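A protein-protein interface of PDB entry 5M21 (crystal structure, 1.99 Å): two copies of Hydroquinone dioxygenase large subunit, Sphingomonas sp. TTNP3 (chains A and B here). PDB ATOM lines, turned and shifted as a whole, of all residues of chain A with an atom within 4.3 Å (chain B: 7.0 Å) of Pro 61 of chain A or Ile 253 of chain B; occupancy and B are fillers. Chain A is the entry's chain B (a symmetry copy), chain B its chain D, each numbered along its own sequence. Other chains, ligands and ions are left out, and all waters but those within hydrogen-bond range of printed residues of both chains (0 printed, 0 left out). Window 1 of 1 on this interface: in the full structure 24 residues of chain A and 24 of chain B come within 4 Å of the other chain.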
ATOM      1  N   TYR A  47     -30.629  -9.347  10.672  1.00  0.00           N
ATOM      2  CA  TYR A  47     -30.397 -10.621   9.965  1.00  0.00           C
ATOM      3  C   TYR A  47     -31.620 -11.203   9.296  1.00  0.00           C
ATOM      4  O   TYR A  47     -31.484 -12.075   8.428  1.00  0.00           O
ATOM      5  CB  TYR A  47     -29.946 -11.712  10.945  1.00  0.00           C
ATOM      6  CG  TYR A  47     -28.536 -11.649  11.430  1.00  0.00           C
ATOM      7  CD1 TYR A  47     -27.472 -11.784  10.536  1.00  0.00           C
ATOM      8  CD2 TYR A  47     -28.240 -11.469  12.806  1.00  0.00           C
ATOM      9  CE1 TYR A  47     -26.166 -11.745  10.983  1.00  0.00           C
ATOM     10  CE2 TYR A  47     -26.887 -11.414  13.273  1.00  0.00           C
ATOM     11  CZ  TYR A  47     -25.858 -11.581  12.340  1.00  0.00           C
ATOM     12  OH  TYR A  47     -24.497 -11.607  12.686  1.00  0.00           O
ATOM     13  N   PHE A  48     -32.799 -10.838   9.768  1.00  0.00           N
ATOM     14  CA  PHE A  48     -34.006 -11.548   9.374  1.00  0.00           C
ATOM     15  C   PHE A  48     -35.150 -10.712   8.782  1.00  0.00           C
ATOM     16  O   PHE A  48     -35.340  -9.533   9.142  1.00  0.00           O
ATOM     17  CB  PHE A  48     -34.553 -12.338  10.600  1.00  0.00           C
ATOM     18  CG  PHE A  48     -33.541 -13.328  11.194  1.00  0.00           C
ATOM     19  CD1 PHE A  48     -33.068 -14.414  10.454  1.00  0.00           C
ATOM     20  CD2 PHE A  48     -33.092 -13.179  12.470  1.00  0.00           C
ATOM     21  CE1 PHE A  48     -32.142 -15.297  10.989  1.00  0.00           C
ATOM     22  CE2 PHE A  48     -32.216 -14.082  13.044  1.00  0.00           C
ATOM     23  CZ  PHE A  48     -31.719 -15.151  12.294  1.00  0.00           C
ATOM     24  N   ILE A  60     -37.402 -15.540   7.790  1.00  0.00           N
ATOM     25  CA  ILE A  60     -36.620 -15.927   6.619  1.00  0.00           C
ATOM     26  C   ILE A  60     -35.310 -15.133   6.705  1.00  0.00           C
ATOM     27  O   ILE A  60     -35.349 -13.998   7.082  1.00  0.00           O
ATOM     28  CB  ILE A  60     -37.405 -15.580   5.344  1.00  0.00           C
ATOM     29  CG1 ILE A  60     -38.767 -16.312   5.373  1.00  0.00           C
ATOM     30  CG2 ILE A  60     -36.592 -15.870   4.082  1.00  0.00           C
ATOM     31  CD1 ILE A  60     -39.616 -16.121   4.118  1.00  0.00           C
ATOM     32  N   PRO A  61     -34.156 -15.716   6.342  1.00  0.00           N
ATOM     33  CA  PRO A  61     -32.968 -14.832   6.444  1.00  0.00           C
ATOM     34  C   PRO A  61     -33.092 -13.667   5.481  1.00  0.00           C
ATOM     35  O   PRO A  61     -33.522 -13.879   4.352  1.00  0.00           O
ATOM     36  CB  PRO A  61     -31.839 -15.714   5.950  1.00  0.00           C
ATOM     37  CG  PRO A  61     -32.281 -17.105   6.286  1.00  0.00           C
ATOM     38  CD  PRO A  61     -33.775 -17.105   6.016  1.00  0.00           C
ATOM     39  N   ILE A  62     -32.670 -12.457   5.869  1.00  0.00           N
ATOM     40  CA  ILE A  62     -32.977 -11.265   5.050  1.00  0.00           C
ATOM     41  C   ILE A  62     -32.385 -11.303   3.611  1.00  0.00           C
ATOM     42  O   ILE A  62     -32.993 -10.788   2.657  1.00  0.00           O
ATOM     43  CB  ILE A  62     -32.677  -9.939   5.829  1.00  0.00           C
ATOM     44  CG1 ILE A  62     -33.416  -8.746   5.185  1.00  0.00           C
ATOM     45  CG2 ILE A  62     -31.156  -9.679   5.985  1.00  0.00           C
ATOM     46  CD1 ILE A  62     -34.905  -8.952   5.028  1.00  0.00           C
ATOM     47  N   ASP A  63     -31.221 -11.932   3.431  1.00  0.00           N
ATOM     48  CA  ASP A  63     -30.652 -12.031   2.099  1.00  0.00           C
ATOM     49  C   ASP A  63     -31.519 -12.837   1.112  1.00  0.00           C
ATOM     50  O   ASP A  63     -31.862 -12.348   0.060  1.00  0.00           O
ATOM     51  CB  ASP A  63     -29.191 -12.489   2.099  1.00  0.00           C
ATOM     52  CG  ASP A  63     -28.999 -13.879   2.726  1.00  0.00           C
ATOM     53  OD1 ASP A  63     -29.883 -14.437   3.435  1.00  0.00           O
ATOM     54  OD2 ASP A  63     -27.910 -14.441   2.506  1.00  0.00           O
ATOM     55  N   ALA A  64     -31.878 -14.049   1.492  1.00  0.00           N
ATOM     56  CA  ALA A  64     -32.818 -14.840   0.729  1.00  0.00           C
ATOM     57  C   ALA A  64     -34.126 -14.128   0.543  1.00  0.00           C
ATOM     58  O   ALA A  64     -34.710 -14.200  -0.544  1.00  0.00           O
ATOM     59  CB  ALA A  64     -33.076 -16.171   1.423  1.00  0.00           C
ATOM     60  N   PHE A  65     -34.645 -13.507   1.597  1.00  0.00           N
ATOM     61  CA  PHE A  65     -35.923 -12.807   1.479  1.00  0.00           C
ATOM     62  C   PHE A  65     -35.946 -11.724   0.379  1.00  0.00           C
ATOM     63  O   PHE A  65     -36.946 -11.563  -0.347  1.00  0.00           O
ATOM     64  CB  PHE A  65     -36.275 -12.108   2.801  1.00  0.00           C
ATOM     65  CG  PHE A  65     -37.610 -11.489   2.777  1.00  0.00           C
ATOM     66  CD1 PHE A  65     -38.717 -12.265   3.051  1.00  0.00           C
ATOM     67  CD2 PHE A  65     -37.760 -10.145   2.477  1.00  0.00           C
ATOM     68  CE1 PHE A  65     -39.988 -11.713   2.986  1.00  0.00           C
ATOM     69  CE2 PHE A  65     -39.025  -9.574   2.390  1.00  0.00           C
ATOM     70  CZ  PHE A  65     -40.140 -10.372   2.649  1.00  0.00           C
ATOM     71  N   ARG B  67     -20.577 -24.097   8.007  1.00  0.00           N
ATOM     72  CA  ARG B  67     -21.068 -23.810   9.333  1.00  0.00           C
ATOM     73  C   ARG B  67     -21.594 -25.070  10.027  1.00  0.00           C
ATOM     74  O   ARG B  67     -21.339 -25.246  11.216  1.00  0.00           O
ATOM     75  CB  ARG B  67     -22.147 -22.705   9.323  1.00  0.00           C
ATOM     76  CG  ARG B  67     -21.460 -21.390   9.053  1.00  0.00           C
ATOM     77  CD  ARG B  67     -22.348 -20.224   9.386  1.00  0.00           C
ATOM     78  NE  ARG B  67     -23.169 -20.004   8.225  1.00  0.00           N
ATOM     79  CZ  ARG B  67     -24.445 -20.316   8.135  1.00  0.00           C
ATOM     80  NH1 ARG B  67     -25.076 -20.853   9.202  1.00  0.00           N
ATOM     81  NH2 ARG B  67     -25.093 -20.036   6.998  1.00  0.00           N
ATOM     82  N   ARG B  71     -19.640 -27.296  13.270  1.00  0.00           N
ATOM     83  CA  ARG B  71     -20.349 -27.857  14.433  1.00  0.00           C
ATOM     84  C   ARG B  71     -20.153 -29.382  14.593  1.00  0.00           C
ATOM     85  O   ARG B  71     -19.661 -29.800  15.609  1.00  0.00           O
ATOM     86  CB  ARG B  71     -21.864 -27.520  14.418  1.00  0.00           C
ATOM     87  CG  ARG B  71     -22.248 -26.019  14.439  1.00  0.00           C
ATOM     88  CD  ARG B  71     -21.287 -25.221  15.300  1.00  0.00           C
ATOM     89  NE  ARG B  71     -21.552 -23.792  15.377  1.00  0.00           N
ATOM     90  CZ  ARG B  71     -21.190 -22.899  14.463  1.00  0.00           C
ATOM     91  NH1 ARG B  71     -20.669 -23.303  13.301  1.00  0.00           N
ATOM     92  NH2 ARG B  71     -21.417 -21.600  14.692  1.00  0.00           N
ATOM     93  N   ALA B 145     -20.721 -15.512  13.658  1.00  0.00           N
ATOM     94  CA  ALA B 145     -21.913 -15.034  12.969  1.00  0.00           C
ATOM     95  C   ALA B 145     -21.554 -14.332  11.668  1.00  0.00           C
ATOM     96  O   ALA B 145     -20.420 -13.837  11.503  1.00  0.00           O
ATOM     97  CB  ALA B 145     -22.750 -14.133  13.849  1.00  0.00           C
ATOM     98  N   PRO B 146     -22.525 -14.254  10.735  1.00  0.00           N
ATOM     99  CA  PRO B 146     -22.189 -13.631   9.441  1.00  0.00           C
ATOM    100  C   PRO B 146     -21.564 -12.201   9.517  1.00  0.00           C
ATOM    101  O   PRO B 146     -20.569 -11.958   8.830  1.00  0.00           O
ATOM    102  CB  PRO B 146     -23.528 -13.672   8.672  1.00  0.00           C
ATOM    103  CG  PRO B 146     -24.212 -14.876   9.278  1.00  0.00           C
ATOM    104  CD  PRO B 146     -23.929 -14.721  10.766  1.00  0.00           C
ATOM    105  N   THR B 231     -20.042 -19.008  18.041  1.00  0.00           N
ATOM    106  CA  THR B 231     -21.483 -19.016  18.268  1.00  0.00           C
ATOM    107  C   THR B 231     -22.007 -20.442  18.231  1.00  0.00           C
ATOM    108  O   THR B 231     -21.390 -21.340  17.606  1.00  0.00           O
ATOM    109  CB  THR B 231     -22.239 -18.204  17.218  1.00  0.00           C
ATOM    110  OG1 THR B 231     -21.940 -18.727  15.896  1.00  0.00           O
ATOM    111  CG2 THR B 231     -21.842 -16.738  17.308  1.00  0.00           C
ATOM    112  N   TRP B 232     -23.169 -20.637  18.844  1.00  0.00           N
ATOM    113  CA  TRP B 232     -23.830 -21.940  18.887  1.00  0.00           C
ATOM    114  C   TRP B 232     -22.868 -23.105  19.200  1.00  0.00           C
ATOM    115  O   TRP B 232     -22.591 -23.953  18.308  1.00  0.00           O
ATOM    116  CB  TRP B 232     -24.522 -22.209  17.557  1.00  0.00           C
ATOM    117  CG  TRP B 232     -25.452 -21.173  17.110  1.00  0.00           C
ATOM    118  CD1 TRP B 232     -25.222 -20.237  16.154  1.00  0.00           C
ATOM    119  CD2 TRP B 232     -26.794 -21.014  17.512  1.00  0.00           C
ATOM    120  NE1 TRP B 232     -26.338 -19.487  15.948  1.00  0.00           N
ATOM    121  CE2 TRP B 232     -27.322 -19.920  16.774  1.00  0.00           C
ATOM    122  CE3 TRP B 232     -27.613 -21.678  18.428  1.00  0.00           C
ATOM    123  CZ2 TRP B 232     -28.634 -19.472  16.912  1.00  0.00           C
ATOM    124  CZ3 TRP B 232     -28.917 -21.237  18.585  1.00  0.00           C
ATOM    125  CH2 TRP B 232     -29.413 -20.129  17.847  1.00  0.00           C
ATOM    126  N   GLU B 250     -25.376 -17.349  21.181  1.00  0.00           N
ATOM    127  CA  GLU B 250     -26.009 -17.685  19.916  1.00  0.00           C
ATOM    128  C   GLU B 250     -26.246 -16.409  19.078  1.00  0.00           C
ATOM    129  O   GLU B 250     -26.810 -15.416  19.588  1.00  0.00           O
ATOM    130  CB  GLU B 250     -27.388 -18.331  20.189  1.00  0.00           C
ATOM    131  CG  GLU B 250     -27.425 -19.255  21.419  1.00  0.00           C
ATOM    132  CD  GLU B 250     -26.531 -20.491  21.307  1.00  0.00           C
ATOM    133  OE1 GLU B 250     -25.301 -20.390  21.128  1.00  0.00           O
ATOM    134  OE2 GLU B 250     -27.058 -21.614  21.445  1.00  0.00           O
ATOM    135  N   GLU B 251     -25.925 -16.484  17.786  1.00  0.00           N
ATOM    136  CA  GLU B 251     -26.180 -15.349  16.873  1.00  0.00           C
ATOM    137  C   GLU B 251     -26.453 -15.894  15.483  1.00  0.00           C
ATOM    138  O   GLU B 251     -25.786 -16.788  15.016  1.00  0.00           O
ATOM    139  CB  GLU B 251     -24.958 -14.372  16.857  1.00  0.00           C
ATOM    140  CG  GLU B 251     -25.226 -12.970  16.271  1.00  0.00           C
ATOM    141  CD  GLU B 251     -23.967 -12.107  16.179  1.00  0.00           C
ATOM    142  OE1 GLU B 251     -23.052 -12.223  17.022  1.00  0.00           O
ATOM    143  OE2 GLU B 251     -23.890 -11.335  15.220  1.00  0.00           O
ATOM    144  N   PHE B 252     -27.500 -15.372  14.840  1.00  0.00           N
ATOM    145  CA  PHE B 252     -27.909 -15.755  13.508  1.00  0.00           C
ATOM    146  C   PHE B 252     -28.745 -17.042  13.588  1.00  0.00           C
ATOM    147  O   PHE B 252     -29.712 -17.098  14.350  1.00  0.00           O
ATOM    148  CB  PHE B 252     -26.732 -15.761  12.481  1.00  0.00           C
ATOM    149  CG  PHE B 252     -27.194 -15.881  11.023  1.00  0.00           C
ATOM    150  CD1 PHE B 252     -28.192 -15.022  10.492  1.00  0.00           C
ATOM    151  CD2 PHE B 252     -26.699 -16.875  10.207  1.00  0.00           C
ATOM    152  CE1 PHE B 252     -28.665 -15.168   9.180  1.00  0.00           C
ATOM    153  CE2 PHE B 252     -27.165 -17.039   8.879  1.00  0.00           C
ATOM    154  CZ  PHE B 252     -28.118 -16.166   8.356  1.00  0.00           C
ATOM    155  N   ILE B 253     -28.394 -18.074  12.823  1.00  0.00           N
ATOM    156  CA  ILE B 253     -29.145 -19.346  12.799  1.00  0.00           C
ATOM    157  C   ILE B 253     -28.269 -20.504  13.281  1.00  0.00           C
ATOM    158  O   ILE B 253     -27.102 -20.636  12.887  1.00  0.00           O
ATOM    159  CB  ILE B 253     -29.603 -19.640  11.354  1.00  0.00           C
ATOM    160  CG1 ILE B 253     -30.495 -18.489  10.843  1.00  0.00           C
ATOM    161  CG2 ILE B 253     -30.381 -20.968  11.276  1.00  0.00           C
ATOM    162  CD1 ILE B 253     -30.943 -18.666   9.405  1.00  0.00           C
ATOM    163  N   LEU B 254     -28.809 -21.328  14.157  1.00  0.00           N
ATOM    164  CA  LEU B 254     -28.157 -22.603  14.487  1.00  0.00           C
ATOM    165  C   LEU B 254     -27.925 -23.326  13.144  1.00  0.00           C
ATOM    166  O   LEU B 254     -28.847 -23.475  12.364  1.00  0.00           O
ATOM    167  CB  LEU B 254     -29.023 -23.463  15.477  1.00  0.00           C
ATOM    168  CG  LEU B 254     -28.492 -24.869  15.784  1.00  0.00           C
ATOM    169  CD1 LEU B 254     -27.132 -24.841  16.505  1.00  0.00           C
ATOM    170  CD2 LEU B 254     -29.491 -25.690  16.571  1.00  0.00           C
ATOM    171  N   PRO B 255     -26.664 -23.700  12.855  1.00  0.00           N
ATOM    172  CA  PRO B 255     -26.311 -24.218  11.533  1.00  0.00           C
ATOM    173  C   PRO B 255     -26.790 -25.641  11.218  1.00  0.00           C
ATOM    174  O   PRO B 255     -26.570 -26.101  10.119  1.00  0.00           O
ATOM    175  CB  PRO B 255     -24.776 -24.256  11.574  1.00  0.00           C
ATOM    176  CG  PRO B 255     -24.351 -23.294  12.647  1.00  0.00           C
ATOM    177  CD  PRO B 255     -25.464 -23.409  13.675  1.00  0.00           C
ATOM    178  N   VAL B 256     -27.336 -26.356  12.183  1.00  0.00           N
ATOM    179  CA  VAL B 256     -27.844 -27.702  11.944  1.00  0.00           C
ATOM    180  C   VAL B 256     -29.250 -27.706  12.497  1.00  0.00           C
ATOM    181  O   VAL B 256     -29.586 -26.793  13.279  1.00  0.00           O
ATOM    182  CB  VAL B 256     -26.934 -28.743  12.636  1.00  0.00           C
ATOM    183  CG1 VAL B 256     -25.462 -28.509  12.251  1.00  0.00           C
ATOM    184  CG2 VAL B 256     -27.055 -28.689  14.167  1.00  0.00           C
ATOM    185  N   GLN B 306     -34.164 -25.957  15.364  1.00  0.00           N
ATOM    186  CA  GLN B 306     -33.162 -25.028  14.804  1.00  0.00           C
ATOM    187  C   GLN B 306     -33.492 -23.612  15.323  1.00  0.00           C
ATOM    188  O   GLN B 306     -34.656 -23.145  15.237  1.00  0.00           O
ATOM    189  CB  GLN B 306     -33.223 -25.023  13.256  1.00  0.00           C
ATOM    190  CG  GLN B 306     -32.009 -24.274  12.629  1.00  0.00           C
ATOM    191  CD  GLN B 306     -31.875 -24.547  11.164  1.00  0.00           C
ATOM    192  OE1 GLN B 306     -32.866 -24.723  10.499  1.00  0.00           O
ATOM    193  NE2 GLN B 306     -30.661 -24.678  10.684  1.00  0.00           N
ATOM    194  N   GLY B 307     -32.498 -22.946  15.886  1.00  0.00           N
ATOM    195  CA  GLY B 307     -32.752 -21.649  16.528  1.00  0.00           C
ATOM    196  C   GLY B 307     -32.342 -20.404  15.727  1.00  0.00           C
ATOM    197  O   GLY B 307     -31.338 -20.420  14.962  1.00  0.00           O
ATOM    198  N   TYR B 308     -33.050 -19.324  15.998  1.00  0.00           N
ATOM    199  CA  TYR B 308     -32.839 -18.061  15.329  1.00  0.00           C
ATOM    200  C   TYR B 308     -32.665 -17.006  16.416  1.00  0.00           C
ATOM    201  O   TYR B 308     -33.559 -16.791  17.207  1.00  0.00           O
ATOM    202  CB  TYR B 308     -34.076 -17.717  14.521  1.00  0.00           C
ATOM    203  CG  TYR B 308     -34.285 -18.647  13.357  1.00  0.00           C
ATOM    204  CD1 TYR B 308     -34.792 -19.921  13.538  1.00  0.00           C
ATOM    205  CD2 TYR B 308     -33.955 -18.242  12.079  1.00  0.00           C
ATOM    206  CE1 TYR B 308     -34.972 -20.780  12.445  1.00  0.00           C
ATOM    207  CE2 TYR B 308     -34.132 -19.075  10.987  1.00  0.00           C
ATOM    208  CZ  TYR B 308     -34.636 -20.338  11.185  1.00  0.00           C
ATOM    209  OH  TYR B 308     -34.778 -21.149  10.099  1.00  0.00           O
ATOM    210  N   SER B 309     -31.493 -16.385  16.440  1.00  0.00           N
ATOM    211  CA  SER B 309     -31.184 -15.336  17.399  1.00  0.00           C
ATOM    212  C   SER B 309     -30.709 -14.072  16.640  1.00  0.00           C
ATOM    213  O   SER B 309     -29.643 -14.066  16.067  1.00  0.00           O
ATOM    214  CB  SER B 309     -30.071 -15.860  18.337  1.00  0.00           C
ATOM    215  OG  SER B 309     -29.964 -15.018  19.480  1.00  0.00           O
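CB of Ala 145 of chain B touches OH of Tyr 47 of chain A (3.3 Å).
CD of Pro 146 of chain B touches OH of Tyr 47 of chain A, 3.7 Å away.
Phe 252 of chain B touches Tyr 47 of chain A.
Phe 252 of chain B touches Phe 48 of chain A.
CG1 of Ile 253 of chain B touches CE1 of Phe 48 of chain A, 3.6 Å away.
Phe 48 of chain A touches Tyr 308 of chain B.
Phe 48 of chain A touches Ser 309 of chain B (CE2 to C, 3.9 Å).
Ile 253 of chain B touches Pro 61 of chain A (CD1 to CG, 3.7 Å).
The backbone carbonyl oxygen (O) of Ser 309 of chain B lies within hydrogen-bond range of the backbone NH (N) of Phe 252 of chain B (2.8 Å).
O of Ile 253 of chain B sits at hydrogen-bond distance from NE1 of Trp 232 of chain B (3.4 Å).
O of Tyr 47 of chain A is in hydrogen-bond range of N of Ile 62 of chain A, 2.8 Å away.
The indole nitrogen (NE1) of Trp 232 of chain B lies within hydrogen-bond range of the backbone carbonyl oxygen (O) of Glu 251 of chain B, 2.9 Å away.
O of Glu 250 of chain B sits at hydrogen-bond distance from OG of Ser 309 of chain B, 3.2 Å away.
OE2 of Glu 251 of chain B sits at hydrogen-bond distance from OH of Tyr 47 of chain A, 2.6 Å away.
No position is printed for both chains.
Of the 9 pairs that touch across the chains among the printed residues, none has its exchanged pair printed and touching as well.
Of chain B, only Ile 253 comes within 4 Å of Pro 61 of chain A.
Ile 253 of chain B touches two residues of chain A.
Of the printed residues of chain A, Tyr 308 of chain B touches Phe 48 (3.6 Å).
Of the printed residues of chain A, Pro 146 of chain B touches Tyr 47.
Of the printed residues of chain B, Tyr 47 of chain A touches Ala 145, Pro 146, Glu 251 and Phe 252.
Printed residues of chain A within 4 Å of Phe 252 of chain B: Tyr 47 (3.3 Å) and Phe 48 (3.5 Å).
Ala 64 of chain A touches none of the printed residues of chain B.
The nearest residue of chain B that does not touch Pro 61 of chain A is Phe 252 of chain B (4.5 Å).
The nearest printed residue of chain A that does not touch Tyr 308 of chain B is Pro 61 of chain A (5.4 Å).
Printed residues of chain A that touch a printed residue of chain B: Tyr 47, Phe 48 and Pro 61.
Among the printed residues, 9 pairs touch across the chains.
Among the printed residues, no Asp or Glu carboxylate lies within 4 Å of a Lys or Arg side-chain nitrogen of the other chain.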
